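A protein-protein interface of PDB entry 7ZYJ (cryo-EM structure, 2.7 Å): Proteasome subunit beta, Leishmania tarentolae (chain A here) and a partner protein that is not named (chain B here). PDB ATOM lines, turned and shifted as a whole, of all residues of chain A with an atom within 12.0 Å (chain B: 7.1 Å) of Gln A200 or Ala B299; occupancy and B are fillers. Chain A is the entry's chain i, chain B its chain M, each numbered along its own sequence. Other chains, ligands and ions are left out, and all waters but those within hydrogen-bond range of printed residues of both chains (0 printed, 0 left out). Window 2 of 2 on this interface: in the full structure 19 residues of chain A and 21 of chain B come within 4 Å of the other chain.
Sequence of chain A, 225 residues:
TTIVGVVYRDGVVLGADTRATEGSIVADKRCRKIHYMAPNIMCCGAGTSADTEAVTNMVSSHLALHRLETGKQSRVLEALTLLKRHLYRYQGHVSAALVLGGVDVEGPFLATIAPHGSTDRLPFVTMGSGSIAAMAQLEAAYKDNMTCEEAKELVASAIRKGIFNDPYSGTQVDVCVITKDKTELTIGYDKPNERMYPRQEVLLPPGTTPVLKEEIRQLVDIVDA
Printed residues of chain A that touch a printed residue of chain B: Tyr A197 and Gln A200. Hydrophobic or aromatic side chains of chain B within 4 Å of the printed part of chain A: Ala B299. Among the printed residues, 6 pairs touch across the chains. Among the printed residues, no Asp or Glu carboxylate lies within 4 Å of a Lys or Arg side-chain nitrogen of the other chain.
Among the printed residues, pairs that only touch across the chains: Gln A200 with Ala B299 (3.2 Å), Tyr A197 with Lys B302 (3.3 Å) and Gln A200 with Met B300 (3.8 Å).
No residue of chain A comes within 4 Å of Thr B297. No residue of chain A comes within 4 Å of Leu B298. No residue of chain A comes within 4 Å of Leu B301. Of chain A, only Tyr A197 comes within 4 Å of Lys B302. Printed residues of chain A within 4 Å of Asn B303: Tyr A197 and Gln A200. Printed residues of chain B within 4 Å of Tyr A197: Ala B299, Lys B302 and Asn B303. Thr B293 touches none of the printed residues of chain A. The nearest residue of chain A that does not touch Ala B299 is Pro A198 (7.6 Å).
The backbone carbonyl oxygen (O) of Ala B299 is in hydrogen-bond range of the side-chain hydroxyl (OH) of Tyr A197. OD1 of Asn B303 sits close to OH of Tyr A197 (3.2 Å). ND2 of Asn B303 sits close to N of Gln A200 (3.1 Å).
The side-chain amide oxygen (OD1) of Asn B303 sits close to the backbone carbonyl oxygen (O) of Ala B299.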
ATOM      1  N   ARG A 195     -28.642   9.084  -0.936  1.00  0.00           N
ATOM      2  CA  ARG A 195     -27.634   9.724  -0.098  1.00  0.00           C
ATOM      3  C   ARG A 195     -26.347   8.911  -0.162  1.00  0.00           C
ATOM      4  O   ARG A 195     -26.258   7.827   0.421  1.00  0.00           O
ATOM      5  CB  ARG A 195     -28.136   9.853   1.338  1.00  0.00           C
ATOM      6  CG  ARG A 195     -27.194  10.606   2.262  1.00  0.00           C
ATOM      7  CD  ARG A 195     -27.778  10.731   3.660  1.00  0.00           C
ATOM      8  NE  ARG A 195     -26.912  11.497   4.549  1.00  0.00           N
ATOM      9  CZ  ARG A 195     -25.987  10.964   5.336  1.00  0.00           C
ATOM     10  NH1 ARG A 195     -25.783   9.657   5.376  1.00  0.00           N
ATOM     11  NH2 ARG A 195     -25.249  11.762   6.102  1.00  0.00           N
ATOM     12  N   MET A 196     -25.352   9.431  -0.871  1.00  0.00           N
ATOM     13  CA  MET A 196     -24.066   8.769  -1.028  1.00  0.00           C
ATOM     14  C   MET A 196     -22.970   9.577  -0.344  1.00  0.00           C
ATOM     15  O   MET A 196     -23.080  10.796  -0.188  1.00  0.00           O
ATOM     16  CB  MET A 196     -23.727   8.577  -2.508  1.00  0.00           C
ATOM     17  CG  MET A 196     -23.584   9.875  -3.287  1.00  0.00           C
ATOM     18  SD  MET A 196     -22.707   9.659  -4.848  1.00  0.00           S
ATOM     19  CE  MET A 196     -24.076   9.561  -5.999  1.00  0.00           C
ATOM     20  N   TYR A 197     -21.901   8.879   0.056  1.00  0.00           N
ATOM     21  CA  TYR A 197     -20.769   9.475   0.757  1.00  0.00           C
ATOM     22  C   TYR A 197     -21.233  10.257   1.981  1.00  0.00           C
ATOM     23  O   TYR A 197     -21.256  11.494   1.954  1.00  0.00           O
ATOM     24  CB  TYR A 197     -19.962  10.381  -0.174  1.00  0.00           C
ATOM     25  CG  TYR A 197     -18.617  10.766   0.393  1.00  0.00           C
ATOM     26  CD1 TYR A 197     -17.596   9.832   0.505  1.00  0.00           C
ATOM     27  CD2 TYR A 197     -18.369  12.062   0.821  1.00  0.00           C
ATOM     28  CE1 TYR A 197     -16.366  10.178   1.025  1.00  0.00           C
ATOM     29  CE2 TYR A 197     -17.142  12.417   1.340  1.00  0.00           C
ATOM     30  CZ  TYR A 197     -16.145  11.473   1.442  1.00  0.00           C
ATOM     31  OH  TYR A 197     -14.920  11.825   1.961  1.00  0.00           O
ATOM     32  N   PRO A 198     -21.628   9.573   3.060  1.00  0.00           N
ATOM     33  CA  PRO A 198     -22.173  10.276   4.230  1.00  0.00           C
ATOM     34  C   PRO A 198     -21.200  11.263   4.857  1.00  0.00           C
ATOM     35  O   PRO A 198     -19.999  11.247   4.570  1.00  0.00           O
ATOM     36  CB  PRO A 198     -22.508   9.132   5.196  1.00  0.00           C
ATOM     37  CG  PRO A 198     -21.569   8.041   4.821  1.00  0.00           C
ATOM     38  CD  PRO A 198     -21.396   8.142   3.329  1.00  0.00           C
ATOM     39  N   ARG A 199     -21.726  12.126   5.724  1.00  0.00           N
ATOM     40  CA  ARG A 199     -20.943  13.202   6.311  1.00  0.00           C
ATOM     41  C   ARG A 199     -19.884  12.651   7.262  1.00  0.00           C
ATOM     42  O   ARG A 199     -19.999  11.544   7.796  1.00  0.00           O
ATOM     43  CB  ARG A 199     -21.858  14.169   7.060  1.00  0.00           C
ATOM     44  CG  ARG A 199     -21.530  15.639   6.869  1.00  0.00           C
ATOM     45  CD  ARG A 199     -22.729  16.507   7.224  1.00  0.00           C
ATOM     46  NE  ARG A 199     -23.895  16.196   6.405  1.00  0.00           N
ATOM     47  CZ  ARG A 199     -24.988  15.595   6.855  1.00  0.00           C
ATOM     48  NH1 ARG A 199     -25.103  15.227   8.121  1.00  0.00           N
ATOM     49  NH2 ARG A 199     -25.991  15.357   6.015  1.00  0.00           N
ATOM     50  N   GLN A 200     -18.832  13.446   7.467  1.00  0.00           N
ATOM     51  CA  GLN A 200     -17.803  13.092   8.439  1.00  0.00           C
ATOM     52  C   GLN A 200     -18.303  13.210   9.873  1.00  0.00           C
ATOM     53  O   GLN A 200     -17.839  12.467  10.745  1.00  0.00           O
ATOM     54  CB  GLN A 200     -16.569  13.978   8.258  1.00  0.00           C
ATOM     55  CG  GLN A 200     -15.590  13.500   7.202  1.00  0.00           C
ATOM     56  CD  GLN A 200     -14.332  14.344   7.163  1.00  0.00           C
ATOM     57  OE1 GLN A 200     -14.193  15.306   7.918  1.00  0.00           O
ATOM     58  NE2 GLN A 200     -13.411  13.991   6.277  1.00  0.00           N
ATOM     59  N   GLU A 201     -19.238  14.128  10.128  1.00  0.00           N
ATOM     60  CA  GLU A 201     -19.735  14.411  11.474  1.00  0.00           C
ATOM     61  C   GLU A 201     -18.586  14.780  12.415  1.00  0.00           C
ATOM     62  O   GLU A 201     -18.286  14.080  13.384  1.00  0.00           O
ATOM     63  CB  GLU A 201     -20.551  13.236  12.027  1.00  0.00           C
ATOM     64  CG  GLU A 201     -21.759  12.821  11.185  1.00  0.00           C
ATOM     65  CD  GLU A 201     -22.672  13.981  10.806  1.00  0.00           C
ATOM     66  OE1 GLU A 201     -22.699  15.002  11.526  1.00  0.00           O
ATOM     67  OE2 GLU A 201     -23.383  13.863   9.787  1.00  0.00           O
ATOM     68  N   VAL A 202     -17.940  15.898  12.103  1.00  0.00           N
ATOM     69  CA  VAL A 202     -16.872  16.421  12.947  1.00  0.00           C
ATOM     70  C   VAL A 202     -17.496  17.058  14.181  1.00  0.00           C
ATOM     71  O   VAL A 202     -18.370  17.925  14.074  1.00  0.00           O
ATOM     72  CB  VAL A 202     -16.008  17.428  12.172  1.00  0.00           C
ATOM     73  CG1 VAL A 202     -15.003  18.092  13.102  1.00  0.00           C
ATOM     74  CG2 VAL A 202     -15.300  16.737  11.017  1.00  0.00           C
ATOM     75  N   LEU A 203     -17.045  16.629  15.355  1.00  0.00           N
ATOM     76  CA  LEU A 203     -17.667  17.021  16.611  1.00  0.00           C
ATOM     77  C   LEU A 203     -17.099  18.340  17.119  1.00  0.00           C
ATOM     78  O   LEU A 203     -15.908  18.627  16.979  1.00  0.00           O
ATOM     79  CB  LEU A 203     -17.474  15.935  17.670  1.00  0.00           C
ATOM     80  CG  LEU A 203     -18.604  14.916  17.846  1.00  0.00           C
ATOM     81  CD1 LEU A 203     -19.865  15.600  18.351  1.00  0.00           C
ATOM     82  CD2 LEU A 203     -18.879  14.158  16.555  1.00  0.00           C
ATOM     83  N   LEU A 204     -17.978  19.144  17.713  1.00  0.00           N
ATOM     84  CA  LEU A 204     -17.602  20.403  18.354  1.00  0.00           C
ATOM     85  C   LEU A 204     -18.068  20.349  19.801  1.00  0.00           C
ATOM     86  O   LEU A 204     -19.265  20.548  20.077  1.00  0.00           O
ATOM     87  CB  LEU A 204     -18.202  21.600  17.626  1.00  0.00           C
ATOM     88  CG  LEU A 204     -17.800  21.752  16.158  1.00  0.00           C
ATOM     89  CD1 LEU A 204     -18.550  22.900  15.511  1.00  0.00           C
ATOM     90  CD2 LEU A 204     -16.299  21.951  16.034  1.00  0.00           C
ATOM     91  N   LEU B 278     -12.470  24.789   9.188  1.00  0.00           N
ATOM     92  CA  LEU B 278     -11.792  23.546   9.528  1.00  0.00           C
ATOM     93  C   LEU B 278     -10.276  23.635   9.447  1.00  0.00           C
ATOM     94  O   LEU B 278      -9.590  22.813  10.064  1.00  0.00           O
ATOM     95  CB  LEU B 278     -12.272  22.414   8.616  1.00  0.00           C
ATOM     96  CG  LEU B 278     -13.768  22.101   8.596  1.00  0.00           C
ATOM     97  CD1 LEU B 278     -14.074  21.093   7.505  1.00  0.00           C
ATOM     98  CD2 LEU B 278     -14.225  21.586   9.950  1.00  0.00           C
ATOM     99  N   MET B 292      -2.796  18.493   8.573  1.00  0.00           N
ATOM    100  CA  MET B 292      -3.487  17.415   7.881  1.00  0.00           C
ATOM    101  C   MET B 292      -2.582  16.714   6.877  1.00  0.00           C
ATOM    102  O   MET B 292      -1.722  17.336   6.250  1.00  0.00           O
ATOM    103  CB  MET B 292      -4.725  17.957   7.168  1.00  0.00           C
ATOM    104  CG  MET B 292      -5.559  18.892   8.019  1.00  0.00           C
ATOM    105  SD  MET B 292      -7.165  19.221   7.281  1.00  0.00           S
ATOM    106  CE  MET B 292      -8.065  17.752   7.767  1.00  0.00           C
ATOM    107  N   THR B 293      -2.792  15.410   6.724  1.00  0.00           N
ATOM    108  CA  THR B 293      -2.069  14.616   5.745  1.00  0.00           C
ATOM    109  C   THR B 293      -2.835  14.620   4.423  1.00  0.00           C
ATOM    110  O   THR B 293      -3.835  15.323   4.261  1.00  0.00           O
ATOM    111  CB  THR B 293      -1.847  13.199   6.270  1.00  0.00           C
ATOM    112  OG1 THR B 293      -3.030  12.418   6.054  1.00  0.00           O
ATOM    113  CG2 THR B 293      -1.532  13.226   7.756  1.00  0.00           C
ATOM    114  N   LYS B 294      -2.361  13.832   3.454  1.00  0.00           N
ATOM    115  CA  LYS B 294      -3.039  13.758   2.164  1.00  0.00           C
ATOM    116  C   LYS B 294      -4.436  13.167   2.301  1.00  0.00           C
ATOM    117  O   LYS B 294      -5.389  13.661   1.690  1.00  0.00           O
ATOM    118  CB  LYS B 294      -2.209  12.933   1.181  1.00  0.00           C
ATOM    119  CG  LYS B 294      -0.904  13.582   0.766  1.00  0.00           C
ATOM    120  CD  LYS B 294      -0.251  12.815  -0.368  1.00  0.00           C
ATOM    121  CE  LYS B 294       0.287  11.479   0.110  1.00  0.00           C
ATOM    122  NZ  LYS B 294       1.033  10.768  -0.964  1.00  0.00           N
ATOM    123  N   GLU B 295      -4.575  12.104   3.098  1.00  0.00           N
ATOM    124  CA  GLU B 295      -5.857  11.415   3.200  1.00  0.00           C
ATOM    125  C   GLU B 295      -6.917  12.293   3.853  1.00  0.00           C
ATOM    126  O   GLU B 295      -8.055  12.363   3.372  1.00  0.00           O
ATOM    127  CB  GLU B 295      -5.689  10.110   3.979  1.00  0.00           C
ATOM    128  CG  GLU B 295      -5.023   8.991   3.192  1.00  0.00           C
ATOM    129  CD  GLU B 295      -3.528   9.189   3.034  1.00  0.00           C
ATOM    130  OE1 GLU B 295      -2.951  10.006   3.783  1.00  0.00           O
ATOM    131  OE2 GLU B 295      -2.929   8.529   2.161  1.00  0.00           O
ATOM    132  N   GLU B 296      -6.568  12.965   4.952  1.00  0.00           N
ATOM    133  CA  GLU B 296      -7.541  13.816   5.631  1.00  0.00           C
ATOM    134  C   GLU B 296      -7.929  15.009   4.768  1.00  0.00           C
ATOM    135  O   GLU B 296      -9.101  15.400   4.732  1.00  0.00           O
ATOM    136  CB  GLU B 296      -6.987  14.276   6.979  1.00  0.00           C
ATOM    137  CG  GLU B 296      -6.118  13.239   7.671  1.00  0.00           C
ATOM    138  CD  GLU B 296      -5.557  13.734   8.990  1.00  0.00           C
ATOM    139  OE1 GLU B 296      -5.569  12.960   9.970  1.00  0.00           O
ATOM    140  OE2 GLU B 296      -5.109  14.897   9.049  1.00  0.00           O
ATOM    141  N   THR B 297      -6.960  15.597   4.063  1.00  0.00           N
ATOM    142  CA  THR B 297      -7.269  16.695   3.153  1.00  0.00           C
ATOM    143  C   THR B 297      -8.188  16.235   2.030  1.00  0.00           C
ATOM    144  O   THR B 297      -9.141  16.937   1.665  1.00  0.00           O
ATOM    145  CB  THR B 297      -5.978  17.281   2.583  1.00  0.00           C
ATOM    146  OG1 THR B 297      -5.173  17.799   3.650  1.00  0.00           O
ATOM    147  CG2 THR B 297      -6.288  18.397   1.603  1.00  0.00           C
ATOM    148  N   LEU B 298      -7.919  15.054   1.469  1.00  0.00           N
ATOM    149  CA  LEU B 298      -8.772  14.518   0.414  1.00  0.00           C
ATOM    150  C   LEU B 298     -10.186  14.272   0.922  1.00  0.00           C
ATOM    151  O   LEU B 298     -11.163  14.580   0.231  1.00  0.00           O
ATOM    152  CB  LEU B 298      -8.167  13.229  -0.142  1.00  0.00           C
ATOM    153  CG  LEU B 298      -8.767  12.692  -1.440  1.00  0.00           C
ATOM    154  CD1 LEU B 298      -8.373  13.569  -2.615  1.00  0.00           C
ATOM    155  CD2 LEU B 298      -8.337  11.253  -1.673  1.00  0.00           C
ATOM    156  N   ALA B 299     -10.315  13.716   2.129  1.00  0.00           N
ATOM    157  CA  ALA B 299     -11.638  13.482   2.700  1.00  0.00           C
ATOM    158  C   ALA B 299     -12.380  14.792   2.942  1.00  0.00           C
ATOM    159  O   ALA B 299     -13.583  14.895   2.671  1.00  0.00           O
ATOM    160  CB  ALA B 299     -11.513  12.683   3.995  1.00  0.00           C
ATOM    161  N   MET B 300     -11.676  15.806   3.453  1.00  0.00           N
ATOM    162  CA  MET B 300     -12.296  17.109   3.669  1.00  0.00           C
ATOM    163  C   MET B 300     -12.778  17.716   2.359  1.00  0.00           C
ATOM    164  O   MET B 300     -13.886  18.263   2.286  1.00  0.00           O
ATOM    165  CB  MET B 300     -11.306  18.046   4.359  1.00  0.00           C
ATOM    166  CG  MET B 300     -11.658  19.516   4.233  1.00  0.00           C
ATOM    167  SD  MET B 300     -10.258  20.588   4.594  1.00  0.00           S
ATOM    168  CE  MET B 300     -10.268  20.548   6.379  1.00  0.00           C
ATOM    169  N   LEU B 301     -11.960  17.627   1.310  1.00  0.00           N
ATOM    170  CA  LEU B 301     -12.356  18.188   0.023  1.00  0.00           C
ATOM    171  C   LEU B 301     -13.521  17.411  -0.579  1.00  0.00           C
ATOM    172  O   LEU B 301     -14.406  17.997  -1.218  1.00  0.00           O
ATOM    173  CB  LEU B 301     -11.156  18.204  -0.923  1.00  0.00           C
ATOM    174  CG  LEU B 301     -11.179  19.240  -2.044  1.00  0.00           C
ATOM    175  CD1 LEU B 301     -11.347  20.635  -1.469  1.00  0.00           C
ATOM    176  CD2 LEU B 301      -9.902  19.155  -2.855  1.00  0.00           C
ATOM    177  N   LYS B 302     -13.544  16.090  -0.378  1.00  0.00           N
ATOM    178  CA  LYS B 302     -14.676  15.290  -0.832  1.00  0.00           C
ATOM    179  C   LYS B 302     -15.958  15.705  -0.122  1.00  0.00           C
ATOM    180  O   LYS B 302     -17.016  15.809  -0.751  1.00  0.00           O
ATOM    181  CB  LYS B 302     -14.395  13.805  -0.607  1.00  0.00           C
ATOM    182  CG  LYS B 302     -13.444  13.194  -1.617  1.00  0.00           C
ATOM    183  CD  LYS B 302     -13.326  11.694  -1.421  1.00  0.00           C
ATOM    184  CE  LYS B 302     -12.251  11.104  -2.316  1.00  0.00           C
ATOM    185  NZ  LYS B 302     -12.111   9.637  -2.117  1.00  0.00           N
ATOM    186  N   ASN B 303     -15.881  15.950   1.189  1.00  0.00           N
ATOM    187  CA  ASN B 303     -17.050  16.453   1.907  1.00  0.00           C
ATOM    188  C   ASN B 303     -17.480  17.814   1.379  1.00  0.00           C
ATOM    189  O   ASN B 303     -18.679  18.081   1.244  1.00  0.00           O
ATOM    190  CB  ASN B 303     -16.771  16.541   3.405  1.00  0.00           C
ATOM    191  CG  ASN B 303     -16.787  15.193   4.081  1.00  0.00           C
ATOM    192  OD1 ASN B 303     -16.233  14.221   3.574  1.00  0.00           O
ATOM    193  ND2 ASN B 303     -17.456  15.120   5.223  1.00  0.00           N
ATOM    194  N   ALA B 304     -16.517  18.693   1.097  1.00  0.00           N
ATOM    195  CA  ALA B 304     -16.859  20.016   0.586  1.00  0.00           C
ATOM    196  C   ALA B 304     -17.600  19.919  -0.742  1.00  0.00           C
ATOM    197  O   ALA B 304     -18.638  20.563  -0.932  1.00  0.00           O
ATOM    198  CB  ALA B 304     -15.598  20.865   0.438  1.00  0.00           C
ATOM    199  N   PHE B 305     -17.092  19.101  -1.668  1.00  0.00           N
ATOM    200  CA  PHE B 305     -17.767  18.942  -2.954  1.00  0.00           C
ATOM    201  C   PHE B 305     -19.119  18.253  -2.806  1.00  0.00           C
ATOM    202  O   PHE B 305     -20.075  18.606  -3.505  1.00  0.00           O
ATOM    203  CB  PHE B 305     -16.875  18.187  -3.938  1.00  0.00           C
ATOM    204  CG  PHE B 305     -15.808  19.041  -4.557  1.00  0.00           C
ATOM    205  CD1 PHE B 305     -16.103  19.850  -5.641  1.00  0.00           C
ATOM    206  CD2 PHE B 305     -14.521  19.047  -4.056  1.00  0.00           C
ATOM    207  CE1 PHE B 305     -15.134  20.642  -6.218  1.00  0.00           C
ATOM    208  CE2 PHE B 305     -13.548  19.841  -4.627  1.00  0.00           C
ATOM    209  CZ  PHE B 305     -13.854  20.637  -5.710  1.00  0.00           C
ATOM    210  N   PHE B 321      -9.789  14.595  -8.836  1.00  0.00           N
ATOM    211  CA  PHE B 321      -8.775  14.973  -7.866  1.00  0.00           C
ATOM    212  C   PHE B 321      -7.393  14.664  -8.421  1.00  0.00           C
ATOM    213  O   PHE B 321      -7.150  13.567  -8.935  1.00  0.00           O
ATOM    214  CB  PHE B 321      -8.956  14.219  -6.543  1.00  0.00           C
ATOM    215  CG  PHE B 321     -10.179  14.615  -5.769  1.00  0.00           C
ATOM    216  CD1 PHE B 321     -10.207  15.798  -5.054  1.00  0.00           C
ATOM    217  CD2 PHE B 321     -11.293  13.796  -5.743  1.00  0.00           C
ATOM    218  CE1 PHE B 321     -11.328  16.161  -4.332  1.00  0.00           C
ATOM    219  CE2 PHE B 321     -12.414  14.156  -5.025  1.00  0.00           C
ATOM    220  CZ  PHE B 321     -12.432  15.339  -4.319  1.00  0.00           C
